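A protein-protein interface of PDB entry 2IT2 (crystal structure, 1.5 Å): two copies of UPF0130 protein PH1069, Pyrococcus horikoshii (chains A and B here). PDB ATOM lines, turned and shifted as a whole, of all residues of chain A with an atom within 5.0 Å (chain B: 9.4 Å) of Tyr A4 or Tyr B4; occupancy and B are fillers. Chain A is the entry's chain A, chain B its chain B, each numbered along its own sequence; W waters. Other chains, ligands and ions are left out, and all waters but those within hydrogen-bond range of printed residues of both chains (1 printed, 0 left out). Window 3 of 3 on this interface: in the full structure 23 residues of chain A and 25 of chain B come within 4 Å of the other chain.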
ATOM      1  N   LEU A   2     -23.424   6.036  18.549  1.00  0.00           N
ATOM      2  CA  LEU A   2     -23.013   7.193  17.772  1.00  0.00           C
ATOM      3  C   LEU A   2     -22.772   6.748  16.335  1.00  0.00           C
ATOM      4  O   LEU A   2     -21.940   5.882  16.077  1.00  0.00           O
ATOM      5  CB  LEU A   2     -21.734   7.799  18.358  1.00  0.00           C
ATOM      6  CG  LEU A   2     -21.839   8.313  19.795  1.00  0.00           C
ATOM      7  CD1 LEU A   2     -20.475   8.801  20.262  1.00  0.00           C
ATOM      8  CD2 LEU A   2     -22.863   9.438  19.865  1.00  0.00           C
ATOM      9  N   LEU A   3     -23.523   7.327  15.406  1.00  0.00           N
ATOM     10  CA  LEU A   3     -23.383   6.986  13.992  1.00  0.00           C
ATOM     11  C   LEU A   3     -22.958   8.226  13.217  1.00  0.00           C
ATOM     12  O   LEU A   3     -23.624   9.257  13.267  1.00  0.00           O
ATOM     13  CB  LEU A   3     -24.712   6.457  13.440  1.00  0.00           C
ATOM     14  CG  LEU A   3     -25.187   5.115  14.015  1.00  0.00           C
ATOM     15  CD1 LEU A   3     -26.675   4.901  13.750  1.00  0.00           C
ATOM     16  CD2 LEU A   3     -24.367   4.001  13.405  1.00  0.00           C
ATOM     17  N   TYR A   4     -21.846   8.121  12.500  1.00  0.00           N
ATOM     18  CA  TYR A   4     -21.341   9.240  11.719  1.00  0.00           C
ATOM     19  C   TYR A   4     -22.367   9.814  10.739  1.00  0.00           C
ATOM     20  O   TYR A   4     -22.443  11.028  10.565  1.00  0.00           O
ATOM     21  CB  TYR A   4     -20.090   8.819  10.943  1.00  0.00           C
ATOM     22  CG  TYR A   4     -18.799   8.832  11.735  1.00  0.00           C
ATOM     23  CD1 TYR A   4     -18.764   8.456  13.073  1.00  0.00           C
ATOM     24  CD2 TYR A   4     -17.597   9.199  11.124  1.00  0.00           C
ATOM     25  CE1 TYR A   4     -17.556   8.444  13.792  1.00  0.00           C
ATOM     26  CE2 TYR A   4     -16.387   9.186  11.825  1.00  0.00           C
ATOM     27  CZ  TYR A   4     -16.371   8.809  13.156  1.00  0.00           C
ATOM     28  OH  TYR A   4     -15.175   8.770  13.848  1.00  0.00           O
ATOM     29  N   MET A   5     -23.153   8.945  10.098  1.00  0.00           N
ATOM     30  CA  MET A   5     -24.149   9.390   9.117  1.00  0.00           C
ATOM     31  C   MET A   5     -25.502   9.785   9.720  1.00  0.00           C
ATOM     32  O   MET A   5     -26.426  10.159   8.994  1.00  0.00           O
ATOM     33  CB  MET A   5     -24.365   8.306   8.038  1.00  0.00           C
ATOM     34  CG  MET A   5     -23.214   8.180   7.020  1.00  0.00           C
ATOM     35  SD  MET A   5     -23.544   7.059   5.597  1.00  0.00           S
ATOM     36  CE  MET A   5     -23.064   5.411   6.383  1.00  0.00           C
ATOM     37  N   ARG A   6     -25.600   9.689  11.041  1.00  0.00           N
ATOM     38  CA  ARG A   6     -26.803  10.042  11.793  1.00  0.00           C
ATOM     39  C   ARG A   6     -26.325  10.791  13.029  1.00  0.00           C
ATOM     40  O   ARG A   6     -26.576  10.379  14.159  1.00  0.00           O
ATOM     41  CB  ARG A   6     -27.555   8.779  12.212  1.00  0.00           C
ATOM     42  CG  ARG A   6     -28.128   7.991  11.049  1.00  0.00           C
ATOM     43  CD  ARG A   6     -29.523   8.476  10.678  1.00  0.00           C
ATOM     44  NE  ARG A   6     -30.547   7.517  11.083  1.00  0.00           N
ATOM     45  CZ  ARG A   6     -31.459   7.002  10.263  1.00  0.00           C
ATOM     46  NH1 ARG A   6     -31.481   7.352   8.983  1.00  0.00           N
ATOM     47  NH2 ARG A   6     -32.351   6.137  10.725  1.00  0.00           N
ATOM     48  N   PHE A   7     -25.618  11.893  12.786  1.00  0.00           N
ATOM     49  CA  PHE A   7     -25.060  12.746  13.840  1.00  0.00           C
ATOM     50  C   PHE A   7     -26.119  13.199  14.843  1.00  0.00           C
ATOM     51  O   PHE A   7     -26.005  12.943  16.043  1.00  0.00           O
ATOM     52  CB  PHE A   7     -24.385  13.972  13.199  1.00  0.00           C
ATOM     53  CG  PHE A   7     -23.779  14.939  14.190  1.00  0.00           C
ATOM     54  CD1 PHE A   7     -22.521  14.707  14.747  1.00  0.00           C
ATOM     55  CD2 PHE A   7     -24.477  16.075  14.570  1.00  0.00           C
ATOM     56  CE1 PHE A   7     -21.977  15.606  15.676  1.00  0.00           C
ATOM     57  CE2 PHE A   7     -23.941  16.969  15.491  1.00  0.00           C
ATOM     58  CZ  PHE A   7     -22.694  16.733  16.043  1.00  0.00           C
ATOM     59  N   LYS A 113     -27.069  16.547   9.996  1.00  0.00           N
ATOM     60  CA  LYS A 113     -27.294  15.178   9.533  1.00  0.00           C
ATOM     61  C   LYS A 113     -26.120  14.230   9.758  1.00  0.00           C
ATOM     62  O   LYS A 113     -26.308  13.116  10.256  1.00  0.00           O
ATOM     63  CB  LYS A 113     -27.670  15.173   8.051  1.00  0.00           C
ATOM     64  CG  LYS A 113     -29.083  15.666   7.778  1.00  0.00           C
ATOM     65  CD  LYS A 113     -29.518  15.301   6.371  1.00  0.00           C
ATOM     66  CE  LYS A 113     -30.972  15.669   6.129  1.00  0.00           C
ATOM     67  NZ  LYS A 113     -31.443  15.174   4.805  1.00  0.00           N
ATOM     68  N   THR A 114     -24.912  14.673   9.412  1.00  0.00           N
ATOM     69  CA  THR A 114     -23.716  13.838   9.549  1.00  0.00           C
ATOM     70  C   THR A 114     -22.566  14.506  10.292  1.00  0.00           C
ATOM     71  O   THR A 114     -22.567  15.720  10.458  1.00  0.00           O
ATOM     72  CB  THR A 114     -23.175  13.435   8.184  1.00  0.00           C
ATOM     73  OG1 THR A 114     -22.552  14.563   7.559  1.00  0.00           O
ATOM     74  CG2 THR A 114     -24.298  12.959   7.317  1.00  0.00           C
ATOM     75  N   LEU A 115     -21.595  13.709  10.725  1.00  0.00           N
ATOM     76  CA  LEU A 115     -20.438  14.255  11.429  1.00  0.00           C
ATOM     77  C   LEU A 115     -19.684  15.221  10.512  1.00  0.00           C
ATOM     78  O   LEU A 115     -19.219  16.276  10.965  1.00  0.00           O
ATOM     79  CB  LEU A 115     -19.511  13.126  11.899  1.00  0.00           C
ATOM     80  CG  LEU A 115     -18.324  13.574  12.759  1.00  0.00           C
ATOM     81  CD1 LEU A 115     -18.840  14.155  14.068  1.00  0.00           C
ATOM     82  CD2 LEU A 115     -17.404  12.405  13.040  1.00  0.00           C
ATOM     83  N   GLU A 116     -19.568  14.889   9.228  1.00  0.00           N
ATOM     84  CA  GLU A 116     -18.884  15.786   8.306  1.00  0.00           C
ATOM     85  C   GLU A 116     -19.577  17.144   8.306  1.00  0.00           C
ATOM     86  O   GLU A 116     -18.907  18.181   8.325  1.00  0.00           O
ATOM     87  CB  GLU A 116     -18.876  15.222   6.883  1.00  0.00           C
ATOM     88  CG  GLU A 116     -18.369  16.221   5.849  1.00  0.00           C
ATOM     89  CD  GLU A 116     -18.246  15.622   4.467  1.00  0.00           C
ATOM     90  OE1 GLU A 116     -19.230  15.023   3.980  1.00  0.00           O
ATOM     91  OE2 GLU A 116     -17.161  15.751   3.864  1.00  0.00           O
ATOM     92  N   LEU B   2     -12.162  16.440   5.814  1.00  0.00           N
ATOM     93  CA  LEU B   2     -12.051  15.493   6.959  1.00  0.00           C
ATOM     94  C   LEU B   2     -12.161  14.049   6.480  1.00  0.00           C
ATOM     95  O   LEU B   2     -13.075  13.701   5.728  1.00  0.00           O
ATOM     96  CB  LEU B   2     -13.151  15.778   7.992  1.00  0.00           C
ATOM     97  CG  LEU B   2     -13.195  14.833   9.199  1.00  0.00           C
ATOM     98  CD1 LEU B   2     -11.940  15.043  10.032  1.00  0.00           C
ATOM     99  CD2 LEU B   2     -14.443  15.085  10.036  1.00  0.00           C
ATOM    100  N   LEU B   3     -11.222  13.214   6.909  1.00  0.00           N
ATOM    101  CA  LEU B   3     -11.219  11.804   6.538  1.00  0.00           C
ATOM    102  C   LEU B   3     -11.704  10.994   7.729  1.00  0.00           C
ATOM    103  O   LEU B   3     -11.000  10.857   8.730  1.00  0.00           O
ATOM    104  CB  LEU B   3      -9.808  11.357   6.149  1.00  0.00           C
ATOM    105  CG  LEU B   3      -9.221  12.003   4.897  1.00  0.00           C
ATOM    106  CD1 LEU B   3      -7.877  11.360   4.581  1.00  0.00           C
ATOM    107  CD2 LEU B   3     -10.187  11.819   3.733  1.00  0.00           C
ATOM    108  N   TYR B   4     -12.915  10.458   7.624  1.00  0.00           N
ATOM    109  CA  TYR B   4     -13.472   9.687   8.724  1.00  0.00           C
ATOM    110  C   TYR B   4     -12.548   8.601   9.239  1.00  0.00           C
ATOM    111  O   TYR B   4     -12.000   7.824   8.458  1.00  0.00           O
ATOM    112  CB  TYR B   4     -14.792   9.029   8.318  1.00  0.00           C
ATOM    113  CG  TYR B   4     -15.998   9.955   8.268  1.00  0.00           C
ATOM    114  CD1 TYR B   4     -15.943  11.268   8.757  1.00  0.00           C
ATOM    115  CD2 TYR B   4     -17.213   9.499   7.756  1.00  0.00           C
ATOM    116  CE1 TYR B   4     -17.085  12.096   8.732  1.00  0.00           C
ATOM    117  CE2 TYR B   4     -18.345  10.308   7.727  1.00  0.00           C
ATOM    118  CZ  TYR B   4     -18.287  11.597   8.211  1.00  0.00           C
ATOM    119  OH  TYR B   4     -19.460  12.333   8.142  1.00  0.00           O
ATOM    120  N   MET B   5     -12.406   8.552  10.562  1.00  0.00           N
ATOM    121  CA  MET B   5     -11.599   7.557  11.276  1.00  0.00           C
ATOM    122  C   MET B   5     -10.081   7.693  11.134  1.00  0.00           C
ATOM    123  O   MET B   5      -9.339   6.859  11.658  1.00  0.00           O
ATOM    124  CB  MET B   5     -12.009   6.107  10.880  1.00  0.00           C
ATOM    125  CG  MET B   5     -13.532   5.695  11.060  1.00  0.00           C
ATOM    126  SD  MET B   5     -14.140   3.962  10.564  1.00  0.00           S
ATOM    127  CE  MET B   5     -13.750   4.019   8.650  1.00  0.00           C
ATOM    128  N   ARG B   6      -9.620   8.711  10.413  1.00  0.00           N
ATOM    129  CA  ARG B   6      -8.185   8.917  10.267  1.00  0.00           C
ATOM    130  C   ARG B   6      -7.528   9.221  11.613  1.00  0.00           C
ATOM    131  O   ARG B   6      -6.428   8.739  11.874  1.00  0.00           O
ATOM    132  CB  ARG B   6      -7.896  10.062   9.299  1.00  0.00           C
ATOM    133  CG  ARG B   6      -7.441   9.586   7.949  1.00  0.00           C
ATOM    134  CD  ARG B   6      -6.170   8.750   8.073  1.00  0.00           C
ATOM    135  NE  ARG B   6      -5.873   8.035   6.836  1.00  0.00           N
ATOM    136  CZ  ARG B   6      -5.418   8.610   5.727  1.00  0.00           C
ATOM    137  NH1 ARG B   6      -5.195   9.916   5.697  1.00  0.00           N
ATOM    138  NH2 ARG B   6      -5.190   7.878   4.645  1.00  0.00           N
ATOM    139  N   PHE B   7      -8.185  10.008  12.469  1.00  0.00           N
ATOM    140  CA  PHE B   7      -7.578  10.334  13.768  1.00  0.00           C
ATOM    141  C   PHE B   7      -7.410   9.078  14.613  1.00  0.00           C
ATOM    142  O   PHE B   7      -6.496   8.983  15.426  1.00  0.00           O
ATOM    143  CB  PHE B   7      -8.397  11.390  14.535  1.00  0.00           C
ATOM    144  CG  PHE B   7      -9.683  10.877  15.127  1.00  0.00           C
ATOM    145  CD1 PHE B   7     -10.857  10.890  14.388  1.00  0.00           C
ATOM    146  CD2 PHE B   7      -9.725  10.417  16.437  1.00  0.00           C
ATOM    147  CE1 PHE B   7     -12.060  10.457  14.954  1.00  0.00           C
ATOM    148  CE2 PHE B   7     -10.919   9.984  17.009  1.00  0.00           C
ATOM    149  CZ  PHE B   7     -12.084  10.005  16.270  1.00  0.00           C
ATOM    150  N   THR B   8      -8.298   8.108  14.418  1.00  0.00           N
ATOM    151  CA  THR B   8      -8.201   6.864  15.161  1.00  0.00           C
ATOM    152  C   THR B   8      -6.991   6.081  14.624  1.00  0.00           C
ATOM    153  O   THR B   8      -6.236   5.458  15.375  1.00  0.00           O
ATOM    154  CB  THR B   8      -9.470   6.004  14.991  1.00  0.00           C
ATOM    155  OG1 THR B   8     -10.622   6.716  15.468  1.00  0.00           O
ATOM    156  CG2 THR B   8      -9.326   4.728  15.774  1.00  0.00           C
ATOM    157  N   GLU B   9      -6.817   6.111  13.309  1.00  0.00           N
ATOM    158  CA  GLU B   9      -5.692   5.427  12.692  1.00  0.00           C
ATOM    159  C   GLU B   9      -4.359   6.047  13.122  1.00  0.00           C
ATOM    160  O   GLU B   9      -3.360   5.347  13.282  1.00  0.00           O
ATOM    161  CB  GLU B   9      -5.830   5.497  11.171  1.00  0.00           C
ATOM    162  CG  GLU B   9      -6.975   4.646  10.630  1.00  0.00           C
ATOM    163  CD  GLU B   9      -7.634   5.226   9.388  1.00  0.00           C
ATOM    164  OE1 GLU B   9      -6.960   5.938   8.616  1.00  0.00           O
ATOM    165  OE2 GLU B   9      -8.836   4.949   9.173  1.00  0.00           O
ATOM    166  N   ASN B  10      -4.362   7.366  13.305  1.00  0.00           N
ATOM    167  CA  ASN B  10      -3.171   8.119  13.696  1.00  0.00           C
ATOM    168  C   ASN B  10      -2.956   8.257  15.205  1.00  0.00           C
ATOM    169  O   ASN B  10      -1.954   8.832  15.638  1.00  0.00           O
ATOM    170  CB  ASN B  10      -3.234   9.528  13.093  1.00  0.00           C
ATOM    171  CG  ASN B  10      -3.077   9.533  11.585  1.00  0.00           C
ATOM    172  OD1 ASN B  10      -2.250   8.810  11.031  1.00  0.00           O
ATOM    173  ND2 ASN B  10      -3.856  10.372  10.913  1.00  0.00           N
ATOM    174  N   ALA B 112      -8.313  12.017  22.046  1.00  0.00           N
ATOM    175  CA  ALA B 112      -9.051  10.771  22.280  1.00  0.00           C
ATOM    176  C   ALA B 112      -8.947   9.841  21.081  1.00  0.00           C
ATOM    177  O   ALA B 112      -8.908  10.289  19.937  1.00  0.00           O
ATOM    178  CB  ALA B 112     -10.530  11.076  22.580  1.00  0.00           C
ATOM    179  N   LYS B 113      -8.921   8.539  21.346  1.00  0.00           N
ATOM    180  CA  LYS B 113      -8.803   7.572  20.263  1.00  0.00           C
ATOM    181  C   LYS B 113     -10.048   7.412  19.372  1.00  0.00           C
ATOM    182  O   LYS B 113      -9.921   7.168  18.167  1.00  0.00           O
ATOM    183  CB  LYS B 113      -8.394   6.216  20.836  1.00  0.00           C
ATOM    184  CG  LYS B 113      -8.142   5.166  19.778  1.00  0.00           C
ATOM    185  CD  LYS B 113      -7.624   3.895  20.404  1.00  0.00           C
ATOM    186  CE  LYS B 113      -7.314   2.858  19.337  1.00  0.00           C
ATOM    187  NZ  LYS B 113      -6.734   1.617  19.922  1.00  0.00           N
ATOM    188  N   THR B 114     -11.238   7.546  19.956  1.00  0.00           N
ATOM    189  CA  THR B 114     -12.486   7.410  19.195  1.00  0.00           C
ATOM    190  C   THR B 114     -13.488   8.463  19.631  1.00  0.00           C
ATOM    191  O   THR B 114     -13.316   9.105  20.667  1.00  0.00           O
ATOM    192  CB  THR B 114     -13.134   6.029  19.413  1.00  0.00           C
ATOM    193  OG1 THR B 114     -13.639   5.938  20.749  1.00  0.00           O
ATOM    194  CG2 THR B 114     -12.118   4.938  19.191  1.00  0.00           C
ATOM    195  N   LEU B 115     -14.540   8.642  18.838  1.00  0.00           N
ATOM    196  CA  LEU B 115     -15.556   9.618  19.175  1.00  0.00           C
ATOM    197  C   LEU B 115     -16.241   9.203  20.471  1.00  0.00           C
ATOM    198  O   LEU B 115     -16.590  10.042  21.298  1.00  0.00           O
ATOM    199  CB  LEU B 115     -16.577   9.737  18.047  1.00  0.00           C
ATOM    200  CG  LEU B 115     -17.703  10.742  18.300  1.00  0.00           C
ATOM    201  CD1 LEU B 115     -17.139  12.152  18.527  1.00  0.00           C
ATOM    202  CD2 LEU B 115     -18.653  10.711  17.099  1.00  0.00           C
ATOM    203  N   GLU B 116     -16.433   7.900  20.647  1.00  0.00           N
ATOM    204  CA  GLU B 116     -17.051   7.424  21.872  1.00  0.00           C
ATOM    205  C   GLU B 116     -16.200   7.743  23.106  1.00  0.00           C
ATOM    206  O   GLU B 116     -16.739   8.101  24.152  1.00  0.00           O
ATOM    207  CB  GLU B 116     -17.284   5.921  21.798  1.00  0.00           C
ATOM    208  CG  GLU B 116     -18.052   5.378  22.987  1.00  0.00           C
ATOM    209  CD  GLU B 116     -18.279   3.896  22.867  1.00  0.00           C
ATOM    210  OE1 GLU B 116     -18.837   3.479  21.832  1.00  0.00           O
ATOM    211  OE2 GLU B 116     -17.897   3.150  23.795  1.00  0.00           O
ATOM    212  N   ASP B 117     -14.878   7.595  22.989  1.00  0.00           N
ATOM    213  CA  ASP B 117     -13.983   7.876  24.112  1.00  0.00           C
ATOM    214  C   ASP B 117     -14.072   9.353  24.451  1.00  0.00           C
ATOM    215  O   ASP B 117     -14.107   9.720  25.616  1.00  0.00           O
ATOM    216  CB  ASP B 117     -12.528   7.513  23.785  1.00  0.00           C
ATOM    217  CG  ASP B 117     -12.322   6.024  23.614  1.00  0.00           C
ATOM    218  OD1 ASP B 117     -12.893   5.254  24.418  1.00  0.00           O
ATOM    219  OD2 ASP B 117     -11.588   5.626  22.684  1.00  0.00           O
ATOM    220  N   ALA B 118     -14.122  10.195  23.424  1.00  0.00           N
ATOM    221  CA  ALA B 118     -14.214  11.630  23.651  1.00  0.00           C
ATOM    222  C   ALA B 118     -15.489  12.002  24.398  1.00  0.00           C
ATOM    223  O   ALA B 118     -15.455  12.763  25.363  1.00  0.00           O
ATOM    224  CB  ALA B 118     -14.152  12.361  22.336  1.00  0.00           C
ATOM    225  N   ILE B 135     -16.079  18.818  22.549  1.00  0.00           N
ATOM    226  CA  ILE B 135     -15.120  18.370  21.551  1.00  0.00           C
ATOM    227  C   ILE B 135     -14.769  19.622  20.764  1.00  0.00           C
ATOM    228  O   ILE B 135     -15.594  20.152  20.025  1.00  0.00           O
ATOM    229  CB  ILE B 135     -15.718  17.309  20.628  1.00  0.00           C
ATOM    230  CG1 ILE B 135     -15.957  16.028  21.442  1.00  0.00           C
ATOM    231  CG2 ILE B 135     -14.795  17.093  19.433  1.00  0.00           C
ATOM    232  CD1 ILE B 135     -16.747  14.961  20.714  1.00  0.00           C
ATOM    233  N   ILE B 138     -11.855  18.161  15.412  1.00  0.00           N
ATOM    234  CA  ILE B 138     -11.703  16.828  14.865  1.00  0.00           C
ATOM    235  C   ILE B 138     -11.008  16.997  13.531  1.00  0.00           C
ATOM    236  O   ILE B 138     -11.559  17.604  12.620  1.00  0.00           O
ATOM    237  CB  ILE B 138     -13.045  16.148  14.624  1.00  0.00           C
ATOM    238  CG1 ILE B 138     -13.869  16.130  15.913  1.00  0.00           C
ATOM    239  CG2 ILE B 138     -12.803  14.733  14.147  1.00  0.00           C
ATOM    240  CD1 ILE B 138     -15.201  15.424  15.761  1.00  0.00           C
ATOM    241  N   SER B 139      -9.795  16.474  13.426  1.00  0.00           N
ATOM    242  CA  SER B 139      -9.016  16.590  12.203  1.00  0.00           C
ATOM    243  C   SER B 139      -8.587  15.197  11.793  1.00  0.00           C
ATOM    244  O   SER B 139      -9.072  14.204  12.348  1.00  0.00           O
ATOM    245  CB  SER B 139      -7.778  17.471  12.452  1.00  0.00           C
ATOM    246  OG  SER B 139      -6.805  16.843  13.281  1.00  0.00           O
ATOM    247  N   ASN B 140      -7.695  15.118  10.814  1.00  0.00           N
ATOM    248  CA  ASN B 140      -7.193  13.829  10.382  1.00  0.00           C
ATOM    249  C   ASN B 140      -6.058  13.363  11.296  1.00  0.00           C
ATOM    250  O   ASN B 140      -5.689  12.193  11.273  1.00  0.00           O
ATOM    251  CB  ASN B 140      -6.706  13.900   8.938  1.00  0.00           C
ATOM    252  CG  ASN B 140      -7.832  14.171   7.955  1.00  0.00           C
ATOM    253  OD1 ASN B 140      -8.976  13.747   8.158  1.00  0.00           O
ATOM    254  ND2 ASN B 140      -7.510  14.868   6.874  1.00  0.00           N
ATOM    255  N   LEU B 143      -8.433  14.102  17.611  1.00  0.00           N
ATOM    256  CA  LEU B 143      -9.706  14.635  18.085  1.00  0.00           C
ATOM    257  C   LEU B 143      -9.374  15.206  19.461  1.00  0.00           C
ATOM    258  O   LEU B 143      -8.943  14.468  20.346  1.00  0.00           O
ATOM    259  CB  LEU B 143     -10.747  13.521  18.237  1.00  0.00           C
ATOM    260  CG  LEU B 143     -12.154  13.943  18.699  1.00  0.00           C
ATOM    261  CD1 LEU B 143     -13.098  12.793  18.420  1.00  0.00           C
ATOM    262  CD2 LEU B 143     -12.202  14.301  20.171  1.00  0.00           C
HETATM  263  O   HOH W   1     -14.707   7.128  16.186  1.00  0.00           O
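N of Glu A116 is in hydrogen-bond range of OH of Tyr B4 (2.8 Å).
Leu A2 touches Leu B115, but with the chains exchanged Leu A115 does not touch Leu B2 (5.0 Å).
Thr A114 touches Tyr B4, but with the chains exchanged Tyr A4 does not touch Thr B114 (6.0 Å).
Leu A115 touches Tyr B4, but with the chains exchanged Tyr A4 does not touch Leu B115 (4.2 Å).
Glu A116 touches Tyr B4, but with the chains exchanged Tyr A4 does not touch Glu B116 (7.0 Å).
10 positions are printed for both chains.
Water W1 bridges OH of Tyr A4 and N of Leu B115.
Of the 21 printed residues of chain B, 3 touch a printed residue of chain A.
Hydrophobic or aromatic side chains of chain B within 4 Å of the printed part of chain A: Tyr B4, Phe B7 and Leu B115.
Among the printed residues, 6 pairs touch across the chains.
Among the printed residues, no Asp or Glu carboxylate lies within 4 Å of a Lys or Arg side-chain nitrogen of the other chain.
Of the printed residues of chain B, Leu A2 touches Leu B115.
Tyr A4 touches just these residues of chain B: Tyr B4 (3.4 Å) and Phe B7 (3.7 Å).
Of the printed residues of chain B, Leu A115 touches Tyr B4 (3.6 Å).
Of the printed residues of chain B, Glu A116 touches Tyr B4.
Of chain A, only Tyr A4, Thr A114, Leu A115 and Glu A116 come within 4 Å of Tyr B4.
Ala B112 touches none of the printed residues of chain A.
Of the printed residues of chain A, Leu B115 touches Leu A2.
The nearest residue of chain B that does not touch Tyr A4 is Leu B115 (4.2 Å).
The nearest printed residue of chain A that does not touch Leu B115 is Tyr A4 (4.2 Å).
N of Leu A115 is in hydrogen-bond range of O of Tyr A4, 2.8 Å away.
The backbone NH of Glu A116 sits close to the side-chain hydroxyl of Thr A114, at 3.4 Å.
Among the printed residues, pairs that only touch across the chains: Leu A2 with Leu B115, Tyr A4 with Tyr B4, Tyr A4 with Phe B7, Thr A114 with Tyr B4 and Leu A115 with Tyr B4.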
